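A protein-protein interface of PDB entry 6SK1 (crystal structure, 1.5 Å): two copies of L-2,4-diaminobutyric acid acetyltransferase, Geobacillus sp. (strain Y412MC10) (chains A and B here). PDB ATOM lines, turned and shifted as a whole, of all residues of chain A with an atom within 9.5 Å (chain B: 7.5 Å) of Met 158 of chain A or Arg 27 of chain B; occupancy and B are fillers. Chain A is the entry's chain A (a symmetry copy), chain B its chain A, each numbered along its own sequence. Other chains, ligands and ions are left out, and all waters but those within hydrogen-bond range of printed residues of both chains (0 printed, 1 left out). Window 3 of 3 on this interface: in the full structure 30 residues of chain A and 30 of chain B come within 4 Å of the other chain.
The side-chain hydroxyl (OG1) of Thr 30 of chain B is in hydrogen-bond range of the backbone carbonyl oxygen (O) of Met 158 of chain A, at 2.6 Å. The side-chain hydroxyl of Tyr 154 of chain A sits at hydrogen-bond distance from the side-chain carboxylate of Asp 55 of chain B, at 2.6 Å. The backbone nitrogen of Pro 160 of chain A sits close to the side-chain hydroxyl of Thr 30 of chain B, 3.2 Å away.
O of Tyr 154 of chain A lies within hydrogen-bond range of N of Glu 168 of chain A (2.8 Å).
Among the printed residues, merely in contact across the chains: Tyr 154 of chain A with Ala 26 of chain B, Met 158 of chain A with Ala 26 of chain B, Met 158 of chain A with Arg 27 of chain B, Met 158 of chain A with Met 51 of chain B, Phe 159 of chain A with Thr 30 of chain B, Phe 159 of chain A with Met 51 of chain B and Pro 160 of chain A with Pro 47 of chain B.
Of the printed residues of chain B, Tyr 154 of chain A touches Ala 26 and Asp 55. Of the printed residues of chain B, Met 158 of chain A touches Ala 26, Arg 27, Thr 30 and Met 51. Printed residues of chain B within 4 Å of Pro 160 of chain A: Thr 30 (3.2 Å) and Pro 47 (3.6 Å). Ala 26 of chain B touches just these residues of chain A: Tyr 154 (3.7 Å) and Met 158 (3.5 Å). Printed residues of chain A within 4 Å of Arg 27 of chain B: Met 158 (3.9 Å). No residue of chain A comes within 4 Å of Asp 28 of chain B. Printed residues of chain A within 4 Å of Asp 55 of chain B: Tyr 154 (2.6 Å). The nearest printed residue of chain B that does not touch Met 158 of chain A is Gly 29 of chain B (5.5 Å). The nearest printed residue of chain A that does not touch Arg 27 of chain B is Tyr 154 of chain A (6.4 Å). The nearest printed residue of chain A that does not touch Met 51 of chain B is Tyr 154 of chain A (4.1 Å).
Hydrophobic or aromatic side chains of chain B within 4 Å of the printed part of chain A: Ala 26, Pro 47 and Met 51. Hydrophobic or aromatic side chains of chain A that line the printed part of chain B: Tyr 154, Met 158, Phe 159 and Pro 160. Along chain A the printed residues that touch a printed residue of chain B span positions 154 to 160.
No position is printed for both chains. Of the 10 pairs that touch across the chains among the printed residues, none has its exchanged pair printed and touching as well.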
ATOM      1  N   VAL A 152       1.317  11.680   4.453  1.00  0.00           N
ATOM      2  CA  VAL A 152       1.542  10.319   4.238  1.00  0.00           C
ATOM      3  C   VAL A 152       0.203   9.763   3.644  1.00  0.00           C
ATOM      4  O   VAL A 152      -1.085  10.038   4.047  1.00  0.00           O
ATOM      5  CB  VAL A 152       2.232   9.528   5.463  1.00  0.00           C
ATOM      6  CG1 VAL A 152       2.600  10.409   6.659  1.00  0.00           C
ATOM      7  CG2 VAL A 152       1.499   8.329   5.833  1.00  0.00           C
ATOM      8  N   GLY A 153       0.584   9.008   2.652  1.00  0.00           N
ATOM      9  CA  GLY A 153      -0.258   8.171   1.910  1.00  0.00           C
ATOM     10  C   GLY A 153       0.170   6.742   2.067  1.00  0.00           C
ATOM     11  O   GLY A 153       0.160   6.220   3.181  1.00  0.00           O
ATOM     12  N   TYR A 154       0.529   6.080   0.976  1.00  0.00           N
ATOM     13  CA  TYR A 154       0.835   4.639   0.989  1.00  0.00           C
ATOM     14  C   TYR A 154       2.296   4.495   0.589  1.00  0.00           C
ATOM     15  O   TYR A 154       2.629   4.671  -0.608  1.00  0.00           O
ATOM     16  CB  TYR A 154      -0.087   3.857   0.018  1.00  0.00           C
ATOM     17  CG  TYR A 154      -1.566   4.137   0.271  1.00  0.00           C
ATOM     18  CD1 TYR A 154      -2.166   3.732   1.434  1.00  0.00           C
ATOM     19  CD2 TYR A 154      -2.280   4.941  -0.533  1.00  0.00           C
ATOM     20  CE1 TYR A 154      -3.441   4.018   1.743  1.00  0.00           C
ATOM     21  CE2 TYR A 154      -3.573   5.274  -0.200  1.00  0.00           C
ATOM     22  CZ  TYR A 154      -4.162   4.733   0.920  1.00  0.00           C
ATOM     23  OH  TYR A 154      -5.467   5.158   1.209  1.00  0.00           O
ATOM     24  N   GLY A 155       3.129   4.105   1.536  1.00  0.00           N
ATOM     25  CA  GLY A 155       4.541   3.957   1.214  1.00  0.00           C
ATOM     26  C   GLY A 155       4.842   2.756   0.375  1.00  0.00           C
ATOM     27  O   GLY A 155       4.108   1.752   0.346  1.00  0.00           O
ATOM     28  N   ALA A 156       5.988   2.765  -0.312  1.00  0.00           N
ATOM     29  CA  ALA A 156       6.455   1.672  -1.071  1.00  0.00           C
ATOM     30  C   ALA A 156       6.431   0.309  -0.393  1.00  0.00           C
ATOM     31  O   ALA A 156       6.072  -0.726  -0.954  1.00  0.00           O
ATOM     32  CB  ALA A 156       7.866   1.953  -1.543  1.00  0.00           C
ATOM     33  N   GLU A 157       6.705   0.351   0.912  1.00  0.00           N
ATOM     34  CA  GLU A 157       6.840  -0.890   1.689  1.00  0.00           C
ATOM     35  C   GLU A 157       5.505  -1.533   1.908  1.00  0.00           C
ATOM     36  O   GLU A 157       5.468  -2.722   2.338  1.00  0.00           O
ATOM     37  CB  GLU A 157       7.561  -0.574   3.047  1.00  0.00           C
ATOM     38  CG  GLU A 157       6.709   0.189   4.048  1.00  0.00           C
ATOM     39  CD  GLU A 157       6.529   1.715   3.770  1.00  0.00           C
ATOM     40  OE1 GLU A 157       7.202   2.319   2.887  1.00  0.00           O
ATOM     41  OE2 GLU A 157       5.667   2.281   4.484  1.00  0.00           O
ATOM     42  N   MET A 158       4.378  -0.873   1.659  1.00  0.00           N
ATOM     43  CA  MET A 158       3.062  -1.450   1.835  1.00  0.00           C
ATOM     44  C   MET A 158       2.703  -2.429   0.742  1.00  0.00           C
ATOM     45  O   MET A 158       1.688  -3.121   0.829  1.00  0.00           O
ATOM     46  CB  MET A 158       1.953  -0.347   1.820  1.00  0.00           C
ATOM     47  CG  MET A 158       2.065   0.476   3.046  1.00  0.00           C
ATOM     48  SD  MET A 158       0.752   1.638   3.215  1.00  0.00           S
ATOM     49  CE  MET A 158      -0.724   0.571   3.300  1.00  0.00           C
ATOM     50  N   PHE A 159       3.372  -2.393  -0.394  1.00  0.00           N
ATOM     51  CA  PHE A 159       3.017  -3.098  -1.619  1.00  0.00           C
ATOM     52  C   PHE A 159       3.601  -4.528  -1.624  1.00  0.00           C
ATOM     53  O   PHE A 159       4.494  -4.790  -0.802  1.00  0.00           O
ATOM     54  CB  PHE A 159       3.474  -2.306  -2.861  1.00  0.00           C
ATOM     55  CG  PHE A 159       2.665  -1.060  -3.065  1.00  0.00           C
ATOM     56  CD1 PHE A 159       2.912   0.101  -2.401  1.00  0.00           C
ATOM     57  CD2 PHE A 159       1.563  -1.068  -3.929  1.00  0.00           C
ATOM     58  CE1 PHE A 159       2.085   1.201  -2.592  1.00  0.00           C
ATOM     59  CE2 PHE A 159       0.747   0.017  -4.067  1.00  0.00           C
ATOM     60  CZ  PHE A 159       0.978   1.151  -3.375  1.00  0.00           C
ATOM     61  N   PRO A 160       3.095  -5.390  -2.455  1.00  0.00           N
ATOM     62  CA  PRO A 160       3.504  -6.770  -2.387  1.00  0.00           C
ATOM     63  C   PRO A 160       4.970  -6.902  -2.721  1.00  0.00           C
ATOM     64  O   PRO A 160       5.519  -6.301  -3.639  1.00  0.00           O
ATOM     65  CB  PRO A 160       2.636  -7.455  -3.395  1.00  0.00           C
ATOM     66  CG  PRO A 160       1.347  -6.617  -3.469  1.00  0.00           C
ATOM     67  CD  PRO A 160       1.885  -5.225  -3.309  1.00  0.00           C
ATOM     68  N   ASP A 161       5.595  -7.876  -2.042  1.00  0.00           N
ATOM     69  CA  ASP A 161       6.992  -8.176  -2.385  1.00  0.00           C
ATOM     70  C   ASP A 161       6.823  -8.842  -3.814  1.00  0.00           C
ATOM     71  O   ASP A 161       5.810  -9.481  -4.243  1.00  0.00           O
ATOM     72  CB  ASP A 161       7.533  -9.253  -1.452  1.00  0.00           C
ATOM     73  CG  ASP A 161       7.729  -8.806  -0.090  1.00  0.00           C
ATOM     74  OD1 ASP A 161       7.715  -7.629   0.339  1.00  0.00           O
ATOM     75  OD2 ASP A 161       7.889  -9.850   0.680  1.00  0.00           O
ATOM     76  N   THR A 163       6.911  -6.904  -6.580  1.00  0.00           N
ATOM     77  CA  THR A 163       6.565  -5.859  -7.505  1.00  0.00           C
ATOM     78  C   THR A 163       6.812  -4.547  -6.863  1.00  0.00           C
ATOM     79  O   THR A 163       6.032  -4.039  -6.058  1.00  0.00           O
ATOM     80  CB  THR A 163       5.097  -6.030  -8.018  1.00  0.00           C
ATOM     81  OG1 THR A 163       4.899  -7.383  -8.518  1.00  0.00           O
ATOM     82  CG2 THR A 163       4.714  -5.021  -8.925  1.00  0.00           C
ATOM     83  N   THR A 164       7.977  -3.956  -7.157  1.00  0.00           N
ATOM     84  CA  THR A 164       8.372  -2.694  -6.619  1.00  0.00           C
ATOM     85  C   THR A 164       7.423  -1.587  -6.992  1.00  0.00           C
ATOM     86  O   THR A 164       7.169  -1.436  -8.194  1.00  0.00           O
ATOM     87  CB  THR A 164       9.796  -2.302  -7.052  1.00  0.00           C
ATOM     88  OG1 THR A 164      10.657  -3.434  -6.904  1.00  0.00           O
ATOM     89  CG2 THR A 164      10.360  -1.127  -6.257  1.00  0.00           C
ATOM     90  N   HIS A 165       6.927  -0.831  -6.026  1.00  0.00           N
ATOM     91  CA  HIS A 165       6.051   0.284  -6.311  1.00  0.00           C
ATOM     92  C   HIS A 165       6.621   1.506  -5.642  1.00  0.00           C
ATOM     93  O   HIS A 165       7.209   1.450  -4.574  1.00  0.00           O
ATOM     94  CB  HIS A 165       4.681  -0.045  -5.637  1.00  0.00           C
ATOM     95  CG  HIS A 165       3.503   0.714  -6.178  1.00  0.00           C
ATOM     96  ND1 HIS A 165       3.224   2.027  -5.897  1.00  0.00           N
ATOM     97  CD2 HIS A 165       2.539   0.294  -7.000  1.00  0.00           C
ATOM     98  CE1 HIS A 165       2.105   2.388  -6.531  1.00  0.00           C
ATOM     99  NE2 HIS A 165       1.696   1.340  -7.203  1.00  0.00           N
ATOM    100  N   GLU A 166       6.363   2.674  -6.268  1.00  0.00           N
ATOM    101  CA  GLU A 166       6.738   3.913  -5.626  1.00  0.00           C
ATOM    102  C   GLU A 166       5.853   4.293  -4.458  1.00  0.00           C
ATOM    103  O   GLU A 166       4.664   3.862  -4.364  1.00  0.00           O
ATOM    104  CB  GLU A 166       6.831   5.033  -6.650  1.00  0.00           C
ATOM    105  CG  GLU A 166       7.974   4.813  -7.652  1.00  0.00           C
ATOM    106  CD  GLU A 166       8.110   5.895  -8.673  1.00  0.00           C
ATOM    107  OE1 GLU A 166       7.713   5.587  -9.818  1.00  0.00           O
ATOM    108  OE2 GLU A 166       8.517   7.037  -8.325  1.00  0.00           O
ATOM    109  N   ASP A 167       6.390   5.127  -3.569  1.00  0.00           N
ATOM    110  CA  ASP A 167       5.597   5.744  -2.566  1.00  0.00           C
ATOM    111  C   ASP A 167       4.472   6.542  -3.263  1.00  0.00           C
ATOM    112  O   ASP A 167       4.596   7.115  -4.341  1.00  0.00           O
ATOM    113  CB  ASP A 167       6.423   6.782  -1.850  1.00  0.00           C
ATOM    114  CG  ASP A 167       7.420   6.214  -0.866  1.00  0.00           C
ATOM    115  OD1 ASP A 167       7.444   5.116  -0.378  1.00  0.00           O
ATOM    116  OD2 ASP A 167       8.265   7.101  -0.345  1.00  0.00           O
ATOM    117  N   GLU A 168       3.334   6.589  -2.551  1.00  0.00           N
ATOM    118  CA  GLU A 168       2.114   7.252  -2.964  1.00  0.00           C
ATOM    119  C   GLU A 168       1.659   8.276  -1.903  1.00  0.00           C
ATOM    120  O   GLU A 168       0.660   8.022  -1.218  1.00  0.00           O
ATOM    121  CB  GLU A 168       1.094   6.132  -3.203  1.00  0.00           C
ATOM    122  CG  GLU A 168       1.276   5.544  -4.628  1.00  0.00           C
ATOM    123  CD  GLU A 168       1.050   6.645  -5.664  1.00  0.00           C
ATOM    124  OE1 GLU A 168       1.870   7.094  -6.259  1.00  0.00           O
ATOM    125  OE2 GLU A 168       0.114   7.301  -5.751  1.00  0.00           O
ATOM    126  N   PRO A 169       2.356   9.400  -1.742  1.00  0.00           N
ATOM    127  CA  PRO A 169       1.876  10.391  -0.784  1.00  0.00           C
ATOM    128  C   PRO A 169       0.524  10.945  -1.152  1.00  0.00           C
ATOM    129  O   PRO A 169       0.164  11.044  -2.345  1.00  0.00           O
ATOM    130  CB  PRO A 169       2.900  11.514  -0.886  1.00  0.00           C
ATOM    131  CG  PRO A 169       3.853  11.144  -1.914  1.00  0.00           C
ATOM    132  CD  PRO A 169       3.580   9.766  -2.396  1.00  0.00           C
ATOM    133  N   ARG B  22     -13.285  -9.141  10.693  1.00  0.00           N
ATOM    134  CA  ARG B  22     -12.980  -7.760  11.001  1.00  0.00           C
ATOM    135  C   ARG B  22     -13.009  -6.914   9.743  1.00  0.00           C
ATOM    136  O   ARG B  22     -12.996  -7.440   8.657  1.00  0.00           O
ATOM    137  CB  ARG B  22     -11.670  -7.610  11.701  1.00  0.00           C
ATOM    138  CG  ARG B  22     -10.546  -8.071  10.884  1.00  0.00           C
ATOM    139  CD  ARG B  22      -9.241  -7.631  11.643  1.00  0.00           C
ATOM    140  NE  ARG B  22      -8.043  -8.045  10.978  1.00  0.00           N
ATOM    141  CZ  ARG B  22      -7.439  -7.361   9.938  1.00  0.00           C
ATOM    142  NH1 ARG B  22      -7.927  -6.188   9.419  1.00  0.00           N
ATOM    143  NH2 ARG B  22      -6.329  -7.866   9.358  1.00  0.00           N
ATOM    144  N   PRO B  24     -11.271  -4.761   6.839  1.00  0.00           N
ATOM    145  CA  PRO B  24      -9.935  -4.525   6.310  1.00  0.00           C
ATOM    146  C   PRO B  24      -9.483  -3.094   6.556  1.00  0.00           C
ATOM    147  O   PRO B  24     -10.317  -2.250   6.687  1.00  0.00           O
ATOM    148  CB  PRO B  24     -10.155  -4.746   4.810  1.00  0.00           C
ATOM    149  CG  PRO B  24     -11.548  -4.219   4.572  1.00  0.00           C
ATOM    150  CD  PRO B  24     -12.339  -4.692   5.807  1.00  0.00           C
ATOM    151  N   GLU B  25      -8.187  -2.881   6.533  1.00  0.00           N
ATOM    152  CA  GLU B  25      -7.510  -1.601   6.630  1.00  0.00           C
ATOM    153  C   GLU B  25      -6.584  -1.478   5.435  1.00  0.00           C
ATOM    154  O   GLU B  25      -6.288  -2.478   4.780  1.00  0.00           O
ATOM    155  CB  GLU B  25      -6.794  -1.464   7.943  1.00  0.00           C
ATOM    156  CG  GLU B  25      -7.742  -1.610   9.125  1.00  0.00           C
ATOM    157  CD  GLU B  25      -8.685  -0.524   9.345  1.00  0.00           C
ATOM    158  OE1 GLU B  25      -9.620  -0.637  10.255  1.00  0.00           O
ATOM    159  OE2 GLU B  25      -8.660   0.528   8.704  1.00  0.00           O
ATOM    160  N   ALA B  26      -6.086  -0.291   5.196  1.00  0.00           N
ATOM    161  CA  ALA B  26      -5.178  -0.126   4.064  1.00  0.00           C
ATOM    162  C   ALA B  26      -3.986  -1.014   4.197  1.00  0.00           C
ATOM    163  O   ALA B  26      -3.473  -1.541   3.216  1.00  0.00           O
ATOM    164  CB  ALA B  26      -4.774   1.365   3.921  1.00  0.00           C
ATOM    165  N   ARG B  27      -3.460  -1.188   5.423  1.00  0.00           N
ATOM    166  CA  ARG B  27      -2.331  -2.070   5.698  1.00  0.00           C
ATOM    167  C   ARG B  27      -2.543  -3.532   5.294  1.00  0.00           C
ATOM    168  O   ARG B  27      -1.598  -4.287   5.194  1.00  0.00           O
ATOM    169  CB  ARG B  27      -1.947  -2.014   7.170  1.00  0.00           C
ATOM    170  CG  ARG B  27      -3.067  -2.280   8.147  1.00  0.00           C
ATOM    171  CD  ARG B  27      -2.751  -1.902   9.574  1.00  0.00           C
ATOM    172  NE  ARG B  27      -2.655  -0.492   9.791  1.00  0.00           N
ATOM    173  CZ  ARG B  27      -2.338   0.040  10.928  1.00  0.00           C
ATOM    174  NH1 ARG B  27      -2.185   1.340  10.986  1.00  0.00           N
ATOM    175  NH2 ARG B  27      -2.232  -0.749  11.985  1.00  0.00           N
ATOM    176  N   ASP B  28      -3.808  -3.914   5.120  1.00  0.00           N
ATOM    177  CA  ASP B  28      -4.175  -5.245   4.663  1.00  0.00           C
ATOM    178  C   ASP B  28      -4.173  -5.406   3.138  1.00  0.00           C
ATOM    179  O   ASP B  28      -4.426  -6.504   2.667  1.00  0.00           O
ATOM    180  CB  ASP B  28      -5.542  -5.617   5.202  1.00  0.00           C
ATOM    181  CG  ASP B  28      -5.601  -5.676   6.696  1.00  0.00           C
ATOM    182  OD1 ASP B  28      -4.772  -6.403   7.308  1.00  0.00           O
ATOM    183  OD2 ASP B  28      -6.530  -5.125   7.285  1.00  0.00           O
ATOM    184  N   GLY B  29      -3.973  -4.325   2.449  1.00  0.00           N
ATOM    185  CA  GLY B  29      -4.167  -4.418   0.993  1.00  0.00           C
ATOM    186  C   GLY B  29      -3.313  -5.465   0.303  1.00  0.00           C
ATOM    187  O   GLY B  29      -3.804  -6.189  -0.537  1.00  0.00           O
ATOM    188  N   THR B  30      -2.044  -5.525   0.659  1.00  0.00           N
ATOM    189  CA  THR B  30      -1.171  -6.548   0.085  1.00  0.00           C
ATOM    190  C   THR B  30      -1.644  -7.992   0.394  1.00  0.00           C
ATOM    191  O   THR B  30      -1.691  -8.821  -0.516  1.00  0.00           O
ATOM    192  CB  THR B  30       0.235  -6.347   0.542  1.00  0.00           C
ATOM    193  OG1 THR B  30       0.742  -5.280  -0.264  1.00  0.00           O
ATOM    194  CG2 THR B  30       1.088  -7.545   0.303  1.00  0.00           C
ATOM    195  N   ARG B  31      -2.040  -8.265   1.642  1.00  0.00           N
ATOM    196  CA  ARG B  31      -2.430  -9.618   1.972  1.00  0.00           C
ATOM    197  C   ARG B  31      -3.759  -9.959   1.351  1.00  0.00           C
ATOM    198  O   ARG B  31      -4.015 -11.124   0.986  1.00  0.00           O
ATOM    199  CB  ARG B  31      -2.449  -9.838   3.462  1.00  0.00           C
ATOM    200  CG  ARG B  31      -1.057 -10.022   4.051  1.00  0.00           C
ATOM    201  CD  ARG B  31      -0.988 -10.498   5.541  1.00  0.00           C
ATOM    202  NE  ARG B  31      -1.964  -9.862   6.382  1.00  0.00           N
ATOM    203  CZ  ARG B  31      -2.503 -10.351   7.516  1.00  0.00           C
ATOM    204  NH1 ARG B  31      -2.309 -11.597   7.940  1.00  0.00           N
ATOM    205  NH2 ARG B  31      -3.385  -9.596   8.161  1.00  0.00           N
ATOM    206  N   VAL B  32      -4.672  -8.970   1.209  1.00  0.00           N
ATOM    207  CA  VAL B  32      -5.911  -9.242   0.470  1.00  0.00           C
ATOM    208  C   VAL B  32      -5.586  -9.486  -1.015  1.00  0.00           C
ATOM    209  O   VAL B  32      -6.161 -10.418  -1.567  1.00  0.00           O
ATOM    210  CB  VAL B  32      -6.885  -8.016   0.639  1.00  0.00           C
ATOM    211  CG1 VAL B  32      -8.045  -8.083  -0.315  1.00  0.00           C
ATOM    212  CG2 VAL B  32      -7.341  -7.927   2.087  1.00  0.00           C
ATOM    213  N   PRO B  47      -3.019  -3.963  -6.145  1.00  0.00           N
ATOM    214  CA  PRO B  47      -2.826  -3.749  -4.739  1.00  0.00           C
ATOM    215  C   PRO B  47      -3.335  -2.455  -4.218  1.00  0.00           C
ATOM    216  O   PRO B  47      -3.975  -2.375  -3.144  1.00  0.00           O
ATOM    217  CB  PRO B  47      -1.290  -3.924  -4.543  1.00  0.00           C
ATOM    218  CG  PRO B  47      -0.890  -4.779  -5.674  1.00  0.00           C
ATOM    219  CD  PRO B  47      -1.792  -4.413  -6.824  1.00  0.00           C
ATOM    220  N   TYR B  50      -6.990  -2.394  -3.332  1.00  0.00           N
ATOM    221  CA  TYR B  50      -7.357  -2.974  -2.083  1.00  0.00           C
ATOM    222  C   TYR B  50      -6.942  -2.115  -0.878  1.00  0.00           C
ATOM    223  O   TYR B  50      -7.646  -2.104   0.128  1.00  0.00           O
ATOM    224  CB  TYR B  50      -6.799  -4.416  -1.977  1.00  0.00           C
ATOM    225  CG  TYR B  50      -7.366  -5.359  -3.034  1.00  0.00           C
ATOM    226  CD1 TYR B  50      -8.644  -5.788  -2.979  1.00  0.00           C
ATOM    227  CD2 TYR B  50      -6.611  -5.752  -4.094  1.00  0.00           C
ATOM    228  CE1 TYR B  50      -9.197  -6.498  -4.012  1.00  0.00           C
ATOM    229  CE2 TYR B  50      -7.146  -6.488  -5.090  1.00  0.00           C
ATOM    230  CZ  TYR B  50      -8.408  -6.880  -5.045  1.00  0.00           C
ATOM    231  OH  TYR B  50      -8.958  -7.626  -6.084  1.00  0.00           O
ATOM    232  N   MET B  51      -5.881  -1.365  -1.009  1.00  0.00           N
ATOM    233  CA  MET B  51      -5.501  -0.363  -0.017  1.00  0.00           C
ATOM    234  C   MET B  51      -6.554   0.695   0.171  1.00  0.00           C
ATOM    235  O   MET B  51      -6.995   1.019   1.280  1.00  0.00           O
ATOM    236  CB  MET B  51      -4.175   0.291  -0.311  1.00  0.00           C
ATOM    237  CG  MET B  51      -3.038  -0.671  -0.298  1.00  0.00           C
ATOM    238  SD  MET B  51      -1.507   0.145  -0.827  1.00  0.00           S
ATOM    239  CE  MET B  51      -0.494  -1.258  -1.071  1.00  0.00           C
ATOM    240  N   GLY B  54      -9.624  -0.430   2.026  1.00  0.00           N
ATOM    241  CA  GLY B  54      -9.385  -0.469   3.441  1.00  0.00           C
ATOM    242  C   GLY B  54      -9.476   0.875   4.058  1.00  0.00           C
ATOM    243  O   GLY B  54      -9.886   0.970   5.231  1.00  0.00           O
ATOM    244  N   ASP B  55      -9.146   1.966   3.383  1.00  0.00           N
ATOM    245  CA  ASP B  55      -9.252   3.280   3.973  1.00  0.00           C
ATOM    246  C   ASP B  55     -10.570   3.948   3.730  1.00  0.00           C
ATOM    247  O   ASP B  55     -10.999   4.837   4.526  1.00  0.00           O
ATOM    248  CB  ASP B  55      -8.173   4.265   3.442  1.00  0.00           C
ATOM    249  CG  ASP B  55      -6.945   4.345   4.294  1.00  0.00           C
ATOM    250  OD1 ASP B  55      -6.992   4.048   5.493  1.00  0.00           O
ATOM    251  OD2 ASP B  55      -5.900   4.714   3.720  1.00  0.00           O
ATOM    252  N   ILE B  70      -5.014 -14.100   6.609  1.00  0.00           N
ATOM    253  CA  ILE B  70      -6.276 -13.695   5.936  1.00  0.00           C
ATOM    254  C   ILE B  70      -6.715 -14.893   5.153  1.00  0.00           C
ATOM    255  O   ILE B  70      -5.996 -15.330   4.222  1.00  0.00           O
ATOM    256  CB  ILE B  70      -6.118 -12.443   5.108  1.00  0.00           C
ATOM    257  CG1 ILE B  70      -5.812 -11.251   6.058  1.00  0.00           C
ATOM    258  CG2 ILE B  70      -7.385 -12.050   4.362  1.00  0.00           C
ATOM    259  CD1 ILE B  70      -5.613  -9.831   5.525  1.00  0.00           C
